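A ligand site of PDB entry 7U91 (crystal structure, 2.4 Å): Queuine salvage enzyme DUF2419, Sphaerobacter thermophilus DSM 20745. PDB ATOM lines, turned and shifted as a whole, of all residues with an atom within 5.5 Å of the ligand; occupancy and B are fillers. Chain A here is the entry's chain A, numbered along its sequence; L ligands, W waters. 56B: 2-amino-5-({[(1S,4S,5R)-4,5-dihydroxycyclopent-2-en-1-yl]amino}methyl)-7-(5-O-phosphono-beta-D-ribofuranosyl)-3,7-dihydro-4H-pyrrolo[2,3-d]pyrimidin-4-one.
The backbone carbonyl oxygen of Phe 229 lies within hydrogen-bond range of a nitrogen (N2) of the ligand (2.8 Å).
The backbone carbonyl oxygen (O) of Asn 72 lies within hydrogen-bond range of an oxygen (O2') of the ligand (3.1 Å).
An oxygen (O2') of the ligand sits at hydrogen-bond distance from the side-chain amino group (NZ) of Lys 199, at 3.1 Å.
An oxygen (OP3) of the ligand is in hydrogen-bond range of the backbone NH (N) of Tyr 93 (2.8 Å).
An oxygen (O4') of the ligand is in hydrogen-bond range of the indole nitrogen of Trp 302 (3.0 Å).
OD1 of Asp 231 sits at hydrogen-bond distance from N2 of the ligand, at 3.3 Å.
A nitrogen (N1) of the ligand is in hydrogen-bond range of the side-chain carboxylate of Asp 298, 2.6 Å away.
An oxygen (OP1) of the ligand is in salt-bridge range of the guanidinium group of Arg 80 (3.4 Å).
The side-chain amide oxygen (OE1) of Gln 306 lies close to an oxygen (OP2) of the ligand, 2.7 Å away.
The side-chain amide oxygen (OD1) of Asn 72 is in hydrogen-bond range of an oxygen (O2') of the ligand (2.8 Å).
Water W3 lies within hydrogen-bond range of OP1 of the ligand (2.4 Å), OH of Tyr 232 (2.4 Å) and NH2 of Arg 80 (3.0 Å).
Water W1 lies within hydrogen-bond range of OP3 of the ligand (2.5 Å), NE2 of Gln 306 (3.0 Å) and O of Asp 91 (3.2 Å).
Water W2 lies within hydrogen-bond range of the side-chain carboxylate of Asp 207 (2.8 Å), the side-chain hydroxyl of Tyr 93 (2.9 Å), a nitrogen (N10) of the ligand (2.9 Å) and the side-chain amide nitrogen of Asn 72 (3.4 Å).
Water W4 lies within hydrogen-bond range of NZ of Lys 199, O3' of the ligand and N of Cys 74.
Pro 46 touches the ligand.
Trp 48 touches the ligand.
CD2 of Phe 75 touches C5' of the ligand (3.6 Å).
CA of Gly 92 touches OP3 of the ligand, 3.5 Å away.
CH2 of Trp 94 touches O11 of the ligand (3.5 Å).
CD1 of Ile 203 touches C4 of the ligand, at 3.9 Å.
Asp 207 touches the ligand (OD1 to C14, 3.5 Å).
Tyr 232 touches the ligand.
Lys 233 touches the ligand (CG to O5', 3.3 Å).
CG2 of Val 234 touches N2 of the ligand, 3.3 Å away.
NE1 of Trp 299 touches C13 of the ligand (3.3 Å).
Of the 30 residues printed, 20 come within 4 Å of the ligand.
NZ of Lys 233 is in hydrogen-bond range of O of Gly 305 (3.0 Å).
The side-chain carboxylate (OD1) of Asp 231 is in hydrogen-bond range of the backbone NH (N) of Val 234, at 3.2 Å.
The side-chain hydroxyl of Tyr 93 lies within hydrogen-bond range of a ring nitrogen (NE2) of His 53, at 2.6 Å.
The side-chain hydroxyl (OH) of Tyr 232 is in hydrogen-bond range of the backbone NH (N) of Phe 75.
The backbone NH (N) of Lys 233 is in hydrogen-bond range of the side-chain carboxylate (OD2) of Asp 231, 3.2 Å away.
The side-chain hydroxyl (OH) of Tyr 315 sits at hydrogen-bond distance from the guanidinium group (NH1) of Arg 80 (2.9 Å).
The indole nitrogen (NE1) of Trp 48 sits at hydrogen-bond distance from the side-chain carboxylate (OD1) of Asp 207, 3.0 Å away.
The side-chain carboxylate of Asp 91 is in salt-bridge range of the guanidinium group of Arg 80, at 3.4 Å.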
ATOM      1  N   PRO A  46     -22.222  11.116  12.453  1.00  0.00           N
ATOM      2  CA  PRO A  46     -20.984  11.731  12.001  1.00  0.00           C
ATOM      3  C   PRO A  46     -21.092  13.254  11.980  1.00  0.00           C
ATOM      4  O   PRO A  46     -22.187  13.830  11.919  1.00  0.00           O
ATOM      5  CB  PRO A  46     -20.767  11.212  10.574  1.00  0.00           C
ATOM      6  CG  PRO A  46     -22.122  10.671  10.163  1.00  0.00           C
ATOM      7  CD  PRO A  46     -22.773  10.198  11.444  1.00  0.00           C
ATOM      8  N   THR A  47     -19.917  13.855  12.007  1.00  0.00           N
ATOM      9  CA  THR A  47     -19.699  15.296  11.863  1.00  0.00           C
ATOM     10  C   THR A  47     -20.018  15.647  10.419  1.00  0.00           C
ATOM     11  O   THR A  47     -19.632  14.880   9.510  1.00  0.00           O
ATOM     12  CB  THR A  47     -18.273  15.645  12.286  1.00  0.00           C
ATOM     13  OG1 THR A  47     -17.372  14.710  11.683  1.00  0.00           O
ATOM     14  CG2 THR A  47     -18.139  15.604  13.791  1.00  0.00           C
ATOM     15  N   TRP A  48     -20.727  16.758  10.240  1.00  0.00           N
ATOM     16  CA  TRP A  48     -21.014  17.322   8.903  1.00  0.00           C
ATOM     17  C   TRP A  48     -19.694  17.346   8.112  1.00  0.00           C
ATOM     18  O   TRP A  48     -18.717  17.979   8.572  1.00  0.00           O
ATOM     19  CB  TRP A  48     -21.679  18.683   9.018  1.00  0.00           C
ATOM     20  CG  TRP A  48     -22.380  19.059   7.755  1.00  0.00           C
ATOM     21  CD1 TRP A  48     -23.633  18.685   7.361  1.00  0.00           C
ATOM     22  CD2 TRP A  48     -21.838  19.876   6.700  1.00  0.00           C
ATOM     23  NE1 TRP A  48     -23.913  19.234   6.134  1.00  0.00           N
ATOM     24  CE2 TRP A  48     -22.836  19.966   5.710  1.00  0.00           C
ATOM     25  CE3 TRP A  48     -20.631  20.539   6.512  1.00  0.00           C
ATOM     26  CZ2 TRP A  48     -22.644  20.698   4.543  1.00  0.00           C
ATOM     27  CZ3 TRP A  48     -20.435  21.257   5.359  1.00  0.00           C
ATOM     28  CH2 TRP A  48     -21.437  21.339   4.389  1.00  0.00           C
ATOM     29  N   ASN A  49     -19.692  16.628   6.989  1.00  0.00           N
ATOM     30  CA  ASN A  49     -18.474  16.205   6.267  1.00  0.00           C
ATOM     31  C   ASN A  49     -17.802  17.415   5.589  1.00  0.00           C
ATOM     32  O   ASN A  49     -18.372  17.909   4.611  1.00  0.00           O
ATOM     33  CB  ASN A  49     -18.823  15.146   5.225  1.00  0.00           C
ATOM     34  CG  ASN A  49     -17.644  14.771   4.348  1.00  0.00           C
ATOM     35  OD1 ASN A  49     -17.077  15.614   3.647  1.00  0.00           O
ATOM     36  ND2 ASN A  49     -17.269  13.511   4.391  1.00  0.00           N
ATOM     37  N   HIS A  53     -17.816  18.631   0.947  1.00  0.00           N
ATOM     38  CA  HIS A  53     -18.713  19.812   0.955  1.00  0.00           C
ATOM     39  C   HIS A  53     -17.887  21.085   0.757  1.00  0.00           C
ATOM     40  O   HIS A  53     -16.827  21.213   1.391  1.00  0.00           O
ATOM     41  CB  HIS A  53     -19.550  19.876   2.245  1.00  0.00           C
ATOM     42  CG  HIS A  53     -20.669  18.898   2.267  1.00  0.00           C
ATOM     43  ND1 HIS A  53     -20.961  18.128   3.384  1.00  0.00           N
ATOM     44  CD2 HIS A  53     -21.556  18.534   1.309  1.00  0.00           C
ATOM     45  CE1 HIS A  53     -21.978  17.347   3.117  1.00  0.00           C
ATOM     46  NE2 HIS A  53     -22.365  17.571   1.851  1.00  0.00           N
ATOM     47  N   ASN A  72     -30.704  17.373  -4.819  1.00  0.00           N
ATOM     48  CA  ASN A  72     -30.335  16.226  -3.954  1.00  0.00           C
ATOM     49  C   ASN A  72     -31.439  15.156  -4.009  1.00  0.00           C
ATOM     50  O   ASN A  72     -32.246  15.057  -3.048  1.00  0.00           O
ATOM     51  CB  ASN A  72     -30.072  16.621  -2.493  1.00  0.00           C
ATOM     52  CG  ASN A  72     -29.553  15.447  -1.680  1.00  0.00           C
ATOM     53  OD1 ASN A  72     -29.377  14.363  -2.214  1.00  0.00           O
ATOM     54  ND2 ASN A  72     -29.307  15.670  -0.390  1.00  0.00           N
ATOM     55  N   PHE A  73     -31.455  14.362  -5.085  1.00  0.00           N
ATOM     56  CA  PHE A  73     -32.410  13.234  -5.262  1.00  0.00           C
ATOM     57  C   PHE A  73     -31.870  12.251  -6.302  1.00  0.00           C
ATOM     58  O   PHE A  73     -30.942  12.598  -7.062  1.00  0.00           O
ATOM     59  CB  PHE A  73     -33.795  13.745  -5.657  1.00  0.00           C
ATOM     60  CG  PHE A  73     -33.856  14.592  -6.913  1.00  0.00           C
ATOM     61  CD1 PHE A  73     -33.935  14.011  -8.165  1.00  0.00           C
ATOM     62  CD2 PHE A  73     -33.850  15.976  -6.830  1.00  0.00           C
ATOM     63  CE1 PHE A  73     -33.993  14.783  -9.311  1.00  0.00           C
ATOM     64  CE2 PHE A  73     -33.894  16.750  -7.978  1.00  0.00           C
ATOM     65  CZ  PHE A  73     -33.968  16.149  -9.208  1.00  0.00           C
ATOM     66  N   CYS A  74     -32.417  11.031  -6.240  1.00  0.00           N
ATOM     67  CA  CYS A  74     -32.500  10.002  -7.311  1.00  0.00           C
ATOM     68  C   CYS A  74     -31.190   9.799  -8.103  1.00  0.00           C
ATOM     69  O   CYS A  74     -31.044  10.391  -9.179  1.00  0.00           O
ATOM     70  CB  CYS A  74     -33.650  10.374  -8.248  1.00  0.00           C
ATOM     71  SG  CYS A  74     -33.986   9.069  -9.441  1.00  0.00           S
ATOM     72  N   PHE A  75     -30.285   8.940  -7.628  1.00  0.00           N
ATOM     73  CA  PHE A  75     -28.939   8.731  -8.226  1.00  0.00           C
ATOM     74  C   PHE A  75     -28.764   7.313  -8.780  1.00  0.00           C
ATOM     75  O   PHE A  75     -27.679   7.044  -9.336  1.00  0.00           O
ATOM     76  CB  PHE A  75     -27.851   9.015  -7.200  1.00  0.00           C
ATOM     77  CG  PHE A  75     -27.919  10.406  -6.630  1.00  0.00           C
ATOM     78  CD1 PHE A  75     -27.681  11.504  -7.438  1.00  0.00           C
ATOM     79  CD2 PHE A  75     -28.256  10.608  -5.302  1.00  0.00           C
ATOM     80  CE1 PHE A  75     -27.764  12.788  -6.921  1.00  0.00           C
ATOM     81  CE2 PHE A  75     -28.328  11.902  -4.794  1.00  0.00           C
ATOM     82  CZ  PHE A  75     -28.095  12.986  -5.599  1.00  0.00           C
ATOM     83  N   ARG A  80     -24.212   2.597 -13.575  1.00  0.00           N
ATOM     84  CA  ARG A  80     -24.102   3.436 -12.355  1.00  0.00           C
ATOM     85  C   ARG A  80     -23.394   4.741 -12.729  1.00  0.00           C
ATOM     86  O   ARG A  80     -22.354   4.684 -13.438  1.00  0.00           O
ATOM     87  CB  ARG A  80     -23.355   2.702 -11.245  1.00  0.00           C
ATOM     88  CG  ARG A  80     -23.436   3.368  -9.870  1.00  0.00           C
ATOM     89  CD  ARG A  80     -24.594   2.913  -8.995  1.00  0.00           C
ATOM     90  NE  ARG A  80     -24.605   3.767  -7.799  1.00  0.00           N
ATOM     91  CZ  ARG A  80     -25.683   4.180  -7.137  1.00  0.00           C
ATOM     92  NH1 ARG A  80     -26.898   3.814  -7.506  1.00  0.00           N
ATOM     93  NH2 ARG A  80     -25.530   4.967  -6.074  1.00  0.00           N
ATOM     94  N   ASP A  91     -19.958   7.953  -6.195  1.00  0.00           N
ATOM     95  CA  ASP A  91     -21.316   7.685  -6.728  1.00  0.00           C
ATOM     96  C   ASP A  91     -22.342   8.213  -5.721  1.00  0.00           C
ATOM     97  O   ASP A  91     -21.946   8.528  -4.566  1.00  0.00           O
ATOM     98  CB  ASP A  91     -21.525   6.189  -7.016  1.00  0.00           C
ATOM     99  CG  ASP A  91     -21.593   5.283  -5.780  1.00  0.00           C
ATOM    100  OD1 ASP A  91     -21.470   5.793  -4.635  1.00  0.00           O
ATOM    101  OD2 ASP A  91     -21.762   4.062  -5.973  1.00  0.00           O
ATOM    102  N   GLY A  92     -23.603   8.281  -6.145  1.00  0.00           N
ATOM    103  CA  GLY A  92     -24.737   8.709  -5.299  1.00  0.00           C
ATOM    104  C   GLY A  92     -24.544  10.148  -4.851  1.00  0.00           C
ATOM    105  O   GLY A  92     -24.004  10.939  -5.623  1.00  0.00           O
ATOM    106  N   TYR A  93     -24.959  10.448  -3.620  1.00  0.00           N
ATOM    107  CA  TYR A  93     -24.829  11.799  -3.014  1.00  0.00           C
ATOM    108  C   TYR A  93     -23.397  12.315  -3.163  1.00  0.00           C
ATOM    109  O   TYR A  93     -23.209  13.449  -3.615  1.00  0.00           O
ATOM    110  CB  TYR A  93     -25.222  11.786  -1.538  1.00  0.00           C
ATOM    111  CG  TYR A  93     -25.091  13.128  -0.870  1.00  0.00           C
ATOM    112  CD1 TYR A  93     -26.024  14.132  -1.089  1.00  0.00           C
ATOM    113  CD2 TYR A  93     -24.005  13.427  -0.054  1.00  0.00           C
ATOM    114  CE1 TYR A  93     -25.898  15.374  -0.501  1.00  0.00           C
ATOM    115  CE2 TYR A  93     -23.865  14.671   0.532  1.00  0.00           C
ATOM    116  CZ  TYR A  93     -24.816  15.650   0.308  1.00  0.00           C
ATOM    117  OH  TYR A  93     -24.685  16.867   0.900  1.00  0.00           O
ATOM    118  N   TRP A  94     -22.396  11.515  -2.784  1.00  0.00           N
ATOM    119  CA  TRP A  94     -20.997  12.005  -2.725  1.00  0.00           C
ATOM    120  C   TRP A  94     -20.557  12.407  -4.143  1.00  0.00           C
ATOM    121  O   TRP A  94     -19.820  13.406  -4.267  1.00  0.00           O
ATOM    122  CB  TRP A  94     -20.053  11.012  -2.037  1.00  0.00           C
ATOM    123  CG  TRP A  94     -20.362  10.796  -0.578  1.00  0.00           C
ATOM    124  CD1 TRP A  94     -20.618   9.607   0.037  1.00  0.00           C
ATOM    125  CD2 TRP A  94     -20.465  11.800   0.464  1.00  0.00           C
ATOM    126  NE1 TRP A  94     -20.859   9.789   1.363  1.00  0.00           N
ATOM    127  CE2 TRP A  94     -20.770  11.116   1.664  1.00  0.00           C
ATOM    128  CE3 TRP A  94     -20.314  13.191   0.500  1.00  0.00           C
ATOM    129  CZ2 TRP A  94     -20.948  11.781   2.881  1.00  0.00           C
ATOM    130  CZ3 TRP A  94     -20.476  13.847   1.705  1.00  0.00           C
ATOM    131  CH2 TRP A  94     -20.782  13.149   2.879  1.00  0.00           C
ATOM    132  N   LYS A 199     -38.730  16.342   2.338  1.00  0.00           N
ATOM    133  CA  LYS A 199     -37.372  15.740   2.458  1.00  0.00           C
ATOM    134  C   LYS A 199     -36.336  16.834   2.176  1.00  0.00           C
ATOM    135  O   LYS A 199     -35.637  17.240   3.126  1.00  0.00           O
ATOM    136  CB  LYS A 199     -37.229  14.507   1.555  1.00  0.00           C
ATOM    137  CG  LYS A 199     -35.811  13.984   1.342  1.00  0.00           C
ATOM    138  CD  LYS A 199     -35.684  13.042   0.144  1.00  0.00           C
ATOM    139  CE  LYS A 199     -34.385  13.202  -0.627  1.00  0.00           C
ATOM    140  NZ  LYS A 199     -34.418  12.493  -1.927  1.00  0.00           N
ATOM    141  N   ILE A 203     -33.721  18.547   4.808  1.00  0.00           N
ATOM    142  CA  ILE A 203     -32.260  18.292   4.625  1.00  0.00           C
ATOM    143  C   ILE A 203     -31.542  19.654   4.581  1.00  0.00           C
ATOM    144  O   ILE A 203     -30.628  19.861   5.398  1.00  0.00           O
ATOM    145  CB  ILE A 203     -31.996  17.408   3.388  1.00  0.00           C
ATOM    146  CG1 ILE A 203     -31.917  15.941   3.778  1.00  0.00           C
ATOM    147  CG2 ILE A 203     -30.721  17.817   2.663  1.00  0.00           C
ATOM    148  CD1 ILE A 203     -31.874  14.995   2.598  1.00  0.00           C
ATOM    149  N   ASP A 207     -28.437  21.023   6.842  1.00  0.00           N
ATOM    150  CA  ASP A 207     -27.141  21.197   6.128  1.00  0.00           C
ATOM    151  C   ASP A 207     -26.594  22.607   6.399  1.00  0.00           C
ATOM    152  O   ASP A 207     -25.349  22.747   6.463  1.00  0.00           O
ATOM    153  CB  ASP A 207     -27.278  20.924   4.622  1.00  0.00           C
ATOM    154  CG  ASP A 207     -27.208  19.458   4.232  1.00  0.00           C
ATOM    155  OD1 ASP A 207     -26.688  18.652   5.041  1.00  0.00           O
ATOM    156  OD2 ASP A 207     -27.667  19.115   3.123  1.00  0.00           O
ATOM    157  N   ALA A 228     -37.136  12.983  10.206  1.00  0.00           N
ATOM    158  CA  ALA A 228     -36.281  12.231   9.257  1.00  0.00           C
ATOM    159  C   ALA A 228     -36.585  12.712   7.832  1.00  0.00           C
ATOM    160  O   ALA A 228     -37.654  13.284   7.593  1.00  0.00           O
ATOM    161  CB  ALA A 228     -36.538  10.752   9.376  1.00  0.00           C
ATOM    162  N   PHE A 229     -35.640  12.468   6.932  1.00  0.00           N
ATOM    163  CA  PHE A 229     -35.733  12.869   5.516  1.00  0.00           C
ATOM    164  C   PHE A 229     -36.094  11.610   4.723  1.00  0.00           C
ATOM    165  O   PHE A 229     -35.279  10.683   4.627  1.00  0.00           O
ATOM    166  CB  PHE A 229     -34.431  13.567   5.125  1.00  0.00           C
ATOM    167  CG  PHE A 229     -33.866  14.451   6.211  1.00  0.00           C
ATOM    168  CD1 PHE A 229     -34.664  15.396   6.851  1.00  0.00           C
ATOM    169  CD2 PHE A 229     -32.533  14.354   6.589  1.00  0.00           C
ATOM    170  CE1 PHE A 229     -34.137  16.199   7.856  1.00  0.00           C
ATOM    171  CE2 PHE A 229     -32.010  15.170   7.580  1.00  0.00           C
ATOM    172  CZ  PHE A 229     -32.812  16.092   8.213  1.00  0.00           C
ATOM    173  N   ALA A 230     -37.337  11.556   4.263  1.00  0.00           N
ATOM    174  CA  ALA A 230     -37.962  10.338   3.704  1.00  0.00           C
ATOM    175  C   ALA A 230     -37.358  10.031   2.332  1.00  0.00           C
ATOM    176  O   ALA A 230     -38.027  10.294   1.332  1.00  0.00           O
ATOM    177  CB  ALA A 230     -39.455  10.512   3.652  1.00  0.00           C
ATOM    178  N   ASP A 231     -36.128   9.492   2.294  1.00  0.00           N
ATOM    179  CA  ASP A 231     -35.397   9.109   1.053  1.00  0.00           C
ATOM    180  C   ASP A 231     -35.501   7.593   0.845  1.00  0.00           C
ATOM    181  O   ASP A 231     -36.493   7.003   1.352  1.00  0.00           O
ATOM    182  CB  ASP A 231     -33.948   9.602   1.102  1.00  0.00           C
ATOM    183  CG  ASP A 231     -33.004   8.707   1.883  1.00  0.00           C
ATOM    184  OD1 ASP A 231     -33.417   8.182   2.940  1.00  0.00           O
ATOM    185  OD2 ASP A 231     -31.865   8.516   1.413  1.00  0.00           O
ATOM    186  N   TYR A 232     -34.543   6.974   0.133  1.00  0.00           N
ATOM    187  CA  TYR A 232     -34.555   5.521  -0.195  1.00  0.00           C
ATOM    188  C   TYR A 232     -33.460   4.736   0.565  1.00  0.00           C
ATOM    189  O   TYR A 232     -33.569   3.491   0.626  1.00  0.00           O
ATOM    190  CB  TYR A 232     -34.533   5.317  -1.720  1.00  0.00           C
ATOM    191  CG  TYR A 232     -33.364   5.889  -2.501  1.00  0.00           C
ATOM    192  CD1 TYR A 232     -32.112   5.306  -2.461  1.00  0.00           C
ATOM    193  CD2 TYR A 232     -33.547   6.974  -3.348  1.00  0.00           C
ATOM    194  CE1 TYR A 232     -31.065   5.803  -3.224  1.00  0.00           C
ATOM    195  CE2 TYR A 232     -32.510   7.481  -4.113  1.00  0.00           C
ATOM    196  CZ  TYR A 232     -31.260   6.888  -4.053  1.00  0.00           C
ATOM    197  OH  TYR A 232     -30.226   7.386  -4.798  1.00  0.00           O
ATOM    198  N   LYS A 233     -32.463   5.416   1.161  1.00  0.00           N
ATOM    199  CA  LYS A 233     -31.355   4.754   1.907  1.00  0.00           C
ATOM    200  C   LYS A 233     -31.778   4.434   3.342  1.00  0.00           C
ATOM    201  O   LYS A 233     -31.459   3.340   3.822  1.00  0.00           O
ATOM    202  CB  LYS A 233     -30.091   5.616   1.904  1.00  0.00           C
ATOM    203  CG  LYS A 233     -29.317   5.580   0.601  1.00  0.00           C
ATOM    204  CD  LYS A 233     -28.906   4.194   0.154  1.00  0.00           C
ATOM    205  CE  LYS A 233     -28.044   3.502   1.188  1.00  0.00           C
ATOM    206  NZ  LYS A 233     -27.554   2.204   0.677  1.00  0.00           N
ATOM    207  N   VAL A 234     -32.441   5.371   4.022  1.00  0.00           N
ATOM    208  CA  VAL A 234     -32.807   5.225   5.464  1.00  0.00           C
ATOM    209  C   VAL A 234     -33.803   4.084   5.636  1.00  0.00           C
ATOM    210  O   VAL A 234     -33.618   3.274   6.545  1.00  0.00           O
ATOM    211  CB  VAL A 234     -33.313   6.542   6.068  1.00  0.00           C
ATOM    212  CG1 VAL A 234     -33.905   6.334   7.456  1.00  0.00           C
ATOM    213  CG2 VAL A 234     -32.197   7.575   6.111  1.00  0.00           C
ATOM    214  N   ASP A 298     -31.571  10.331  11.848  1.00  0.00           N
ATOM    215  CA  ASP A 298     -31.564  10.206  10.373  1.00  0.00           C
ATOM    216  C   ASP A 298     -30.125  10.166   9.853  1.00  0.00           C
ATOM    217  O   ASP A 298     -29.799   9.220   9.114  1.00  0.00           O
ATOM    218  CB  ASP A 298     -32.377  11.324   9.697  1.00  0.00           C
ATOM    219  CG  ASP A 298     -32.303  11.245   8.191  1.00  0.00           C
ATOM    220  OD1 ASP A 298     -31.219  11.494   7.647  1.00  0.00           O
ATOM    221  OD2 ASP A 298     -33.336  10.888   7.572  1.00  0.00           O
ATOM    222  N   TRP A 299     -29.302  11.158  10.202  1.00  0.00           N
ATOM    223  CA  TRP A 299     -27.873  11.272   9.774  1.00  0.00           C
ATOM    224  C   TRP A 299     -27.122   9.964  10.092  1.00  0.00           C
ATOM    225  O   TRP A 299     -26.328   9.504   9.252  1.00  0.00           O
ATOM    226  CB  TRP A 299     -27.179  12.431  10.482  1.00  0.00           C
ATOM    227  CG  TRP A 299     -27.426  13.776   9.869  1.00  0.00           C
ATOM    228  CD1 TRP A 299     -28.168  14.073   8.766  1.00  0.00           C
ATOM    229  CD2 TRP A 299     -26.873  15.022  10.333  1.00  0.00           C
ATOM    230  NE1 TRP A 299     -28.132  15.417   8.524  1.00  0.00           N
ATOM    231  CE2 TRP A 299     -27.354  16.032   9.468  1.00  0.00           C
ATOM    232  CE3 TRP A 299     -26.053  15.381  11.403  1.00  0.00           C
ATOM    233  CZ2 TRP A 299     -27.008  17.374   9.630  1.00  0.00           C
ATOM    234  CZ3 TRP A 299     -25.718  16.704  11.564  1.00  0.00           C
ATOM    235  CH2 TRP A 299     -26.194  17.681  10.693  1.00  0.00           C
ATOM    236  N   TRP A 302     -28.485   7.145   7.932  1.00  0.00           N
ATOM    237  CA  TRP A 302     -28.020   7.375   6.542  1.00  0.00           C
ATOM    238  C   TRP A 302     -26.566   6.917   6.437  1.00  0.00           C
ATOM    239  O   TRP A 302     -26.215   6.258   5.444  1.00  0.00           O
ATOM    240  CB  TRP A 302     -28.184   8.820   6.057  1.00  0.00           C
ATOM    241  CG  TRP A 302     -27.951   8.968   4.581  1.00  0.00           C
ATOM    242  CD1 TRP A 302     -28.873   8.823   3.587  1.00  0.00           C
ATOM    243  CD2 TRP A 302     -26.700   9.262   3.923  1.00  0.00           C
ATOM    244  NE1 TRP A 302     -28.285   9.024   2.360  1.00  0.00           N
ATOM    245  CE2 TRP A 302     -26.957   9.299   2.544  1.00  0.00           C
ATOM    246  CE3 TRP A 302     -25.403   9.503   4.376  1.00  0.00           C
ATOM    247  CZ2 TRP A 302     -25.967   9.560   1.603  1.00  0.00           C
ATOM    248  CZ3 TRP A 302     -24.422   9.778   3.450  1.00  0.00           C
ATOM    249  CH2 TRP A 302     -24.705   9.804   2.082  1.00  0.00           C
ATOM    250  N   GLY A 305     -26.132   3.267   6.092  1.00  0.00           N
ATOM    251  CA  GLY A 305     -26.525   2.922   4.712  1.00  0.00           C
ATOM    252  C   GLY A 305     -25.334   2.896   3.769  1.00  0.00           C
ATOM    253  O   GLY A 305     -25.379   2.146   2.768  1.00  0.00           O
ATOM    254  N   GLN A 306     -24.308   3.691   4.074  1.00  0.00           N
ATOM    255  CA  GLN A 306     -23.091   3.825   3.231  1.00  0.00           C
ATOM    256  C   GLN A 306     -22.225   2.570   3.359  1.00  0.00           C
ATOM    257  O   GLN A 306     -21.337   2.411   2.539  1.00  0.00           O
ATOM    258  CB  GLN A 306     -22.298   5.099   3.560  1.00  0.00           C
ATOM    259  CG  GLN A 306     -23.012   6.401   3.171  1.00  0.00           C
ATOM    260  CD  GLN A 306     -23.390   6.462   1.708  1.00  0.00           C
ATOM    261  OE1 GLN A 306     -24.571   6.536   1.365  1.00  0.00           O
ATOM    262  NE2 GLN A 306     -22.392   6.429   0.838  1.00  0.00           N
ATOM    263  N   TYR A 315     -32.608  -1.001  -2.104  1.00  0.00           N
ATOM    264  CA  TYR A 315     -33.436   0.196  -1.821  1.00  0.00           C
ATOM    265  C   TYR A 315     -34.516   0.288  -2.900  1.00  0.00           C
ATOM    266  O   TYR A 315     -34.280  -0.172  -4.039  1.00  0.00           O
ATOM    267  CB  TYR A 315     -32.606   1.485  -1.739  1.00  0.00           C
ATOM    268  CG  TYR A 315     -31.605   1.714  -2.840  1.00  0.00           C
ATOM    269  CD1 TYR A 315     -32.004   2.086  -4.118  1.00  0.00           C
ATOM    270  CD2 TYR A 315     -30.239   1.587  -2.612  1.00  0.00           C
ATOM    271  CE1 TYR A 315     -31.080   2.307  -5.135  1.00  0.00           C
ATOM    272  CE2 TYR A 315     -29.305   1.801  -3.611  1.00  0.00           C
ATOM    273  CZ  TYR A 315     -29.730   2.161  -4.878  1.00  0.00           C
ATOM    274  OH  TYR A 315     -28.823   2.370  -5.874  1.00  0.00           O
HETATM  275  N9  56B L   1     -29.626  11.633   1.173  1.00  0.00           N
HETATM  276  C2' 56B L   1     -30.412  11.595  -1.324  1.00  0.00           C
HETATM  277  O2' 56B L   1     -31.402  12.575  -1.368  1.00  0.00           O
HETATM  278  P   56B L   1     -26.408   7.112  -1.894  1.00  0.00           P
HETATM  279  C1' 56B L   1     -30.390  10.969   0.067  1.00  0.00           C
HETATM  280  N10 56B L   1     -26.480  14.221   3.855  1.00  0.00           N
HETATM  281  O11 56B L   1     -23.288  13.251   5.391  1.00  0.00           O
HETATM  282  C8  56B L   1     -28.345  12.249   1.060  1.00  0.00           C
HETATM  283  N3  56B L   1     -31.124  11.103   3.102  1.00  0.00           N
HETATM  284  O12 56B L   1     -24.349  13.022   8.143  1.00  0.00           O
HETATM  285  C7  56B L   1     -27.893  12.675   2.318  1.00  0.00           C
HETATM  286  N2  56B L   1     -32.496  10.645   4.966  1.00  0.00           N
HETATM  287  O6  56B L   1     -28.457  12.874   5.494  1.00  0.00           O
HETATM  288  C9  56B L   1     -26.591  13.405   2.600  1.00  0.00           C
HETATM  289  N1  56B L   1     -30.418  11.790   5.222  1.00  0.00           N
HETATM  290  O4' 56B L   1     -29.744   9.758  -0.125  1.00  0.00           O
HETATM  291  C10 56B L   1     -25.204  14.470   4.615  1.00  0.00           C
HETATM  292  O5' 56B L   1     -28.094   7.850  -1.464  1.00  0.00           O
HETATM  293  C11 56B L   1     -24.671  13.263   5.506  1.00  0.00           C
HETATM  294  OP2 56B L   1     -26.287   6.153  -0.732  1.00  0.00           O
HETATM  295  C12 56B L   1     -25.157  13.527   7.044  1.00  0.00           C
HETATM  296  C13 56B L   1     -25.275  15.034   6.968  1.00  0.00           C
HETATM  297  OP1 56B L   1     -26.739   6.480  -3.225  1.00  0.00           O
HETATM  298  C14 56B L   1     -25.307  15.512   5.720  1.00  0.00           C
HETATM  299  O3' 56B L   1     -32.250  10.083  -1.905  1.00  0.00           O
HETATM  300  C5  56B L   1     -28.946  12.271   3.240  1.00  0.00           C
HETATM  301  C4  56B L   1     -29.975  11.622   2.528  1.00  0.00           C
HETATM  302  C2  56B L   1     -31.326  11.199   4.448  1.00  0.00           C
HETATM  303  C6  56B L   1     -29.214  12.343   4.679  1.00  0.00           C
HETATM  304  C4' 56B L   1     -30.028   9.174  -1.409  1.00  0.00           C
HETATM  305  C5' 56B L   1     -28.679   8.802  -2.175  1.00  0.00           C
HETATM  306  C3' 56B L   1     -30.870  10.294  -2.089  1.00  0.00           C
HETATM  307  OP3 56B L   1     -25.468   8.307  -1.889  1.00  0.00           O
HETATM  308  O   HOH W   1     -22.947   8.188  -1.570  1.00  0.00           O
HETATM  309  O   HOH W   2     -27.283  16.512   2.183  1.00  0.00           O
HETATM  310  O   HOH W   3     -28.204   6.037  -5.096  1.00  0.00           O
HETATM  311  O   HOH W   4     -34.629  10.227  -3.805  1.00  0.00           O
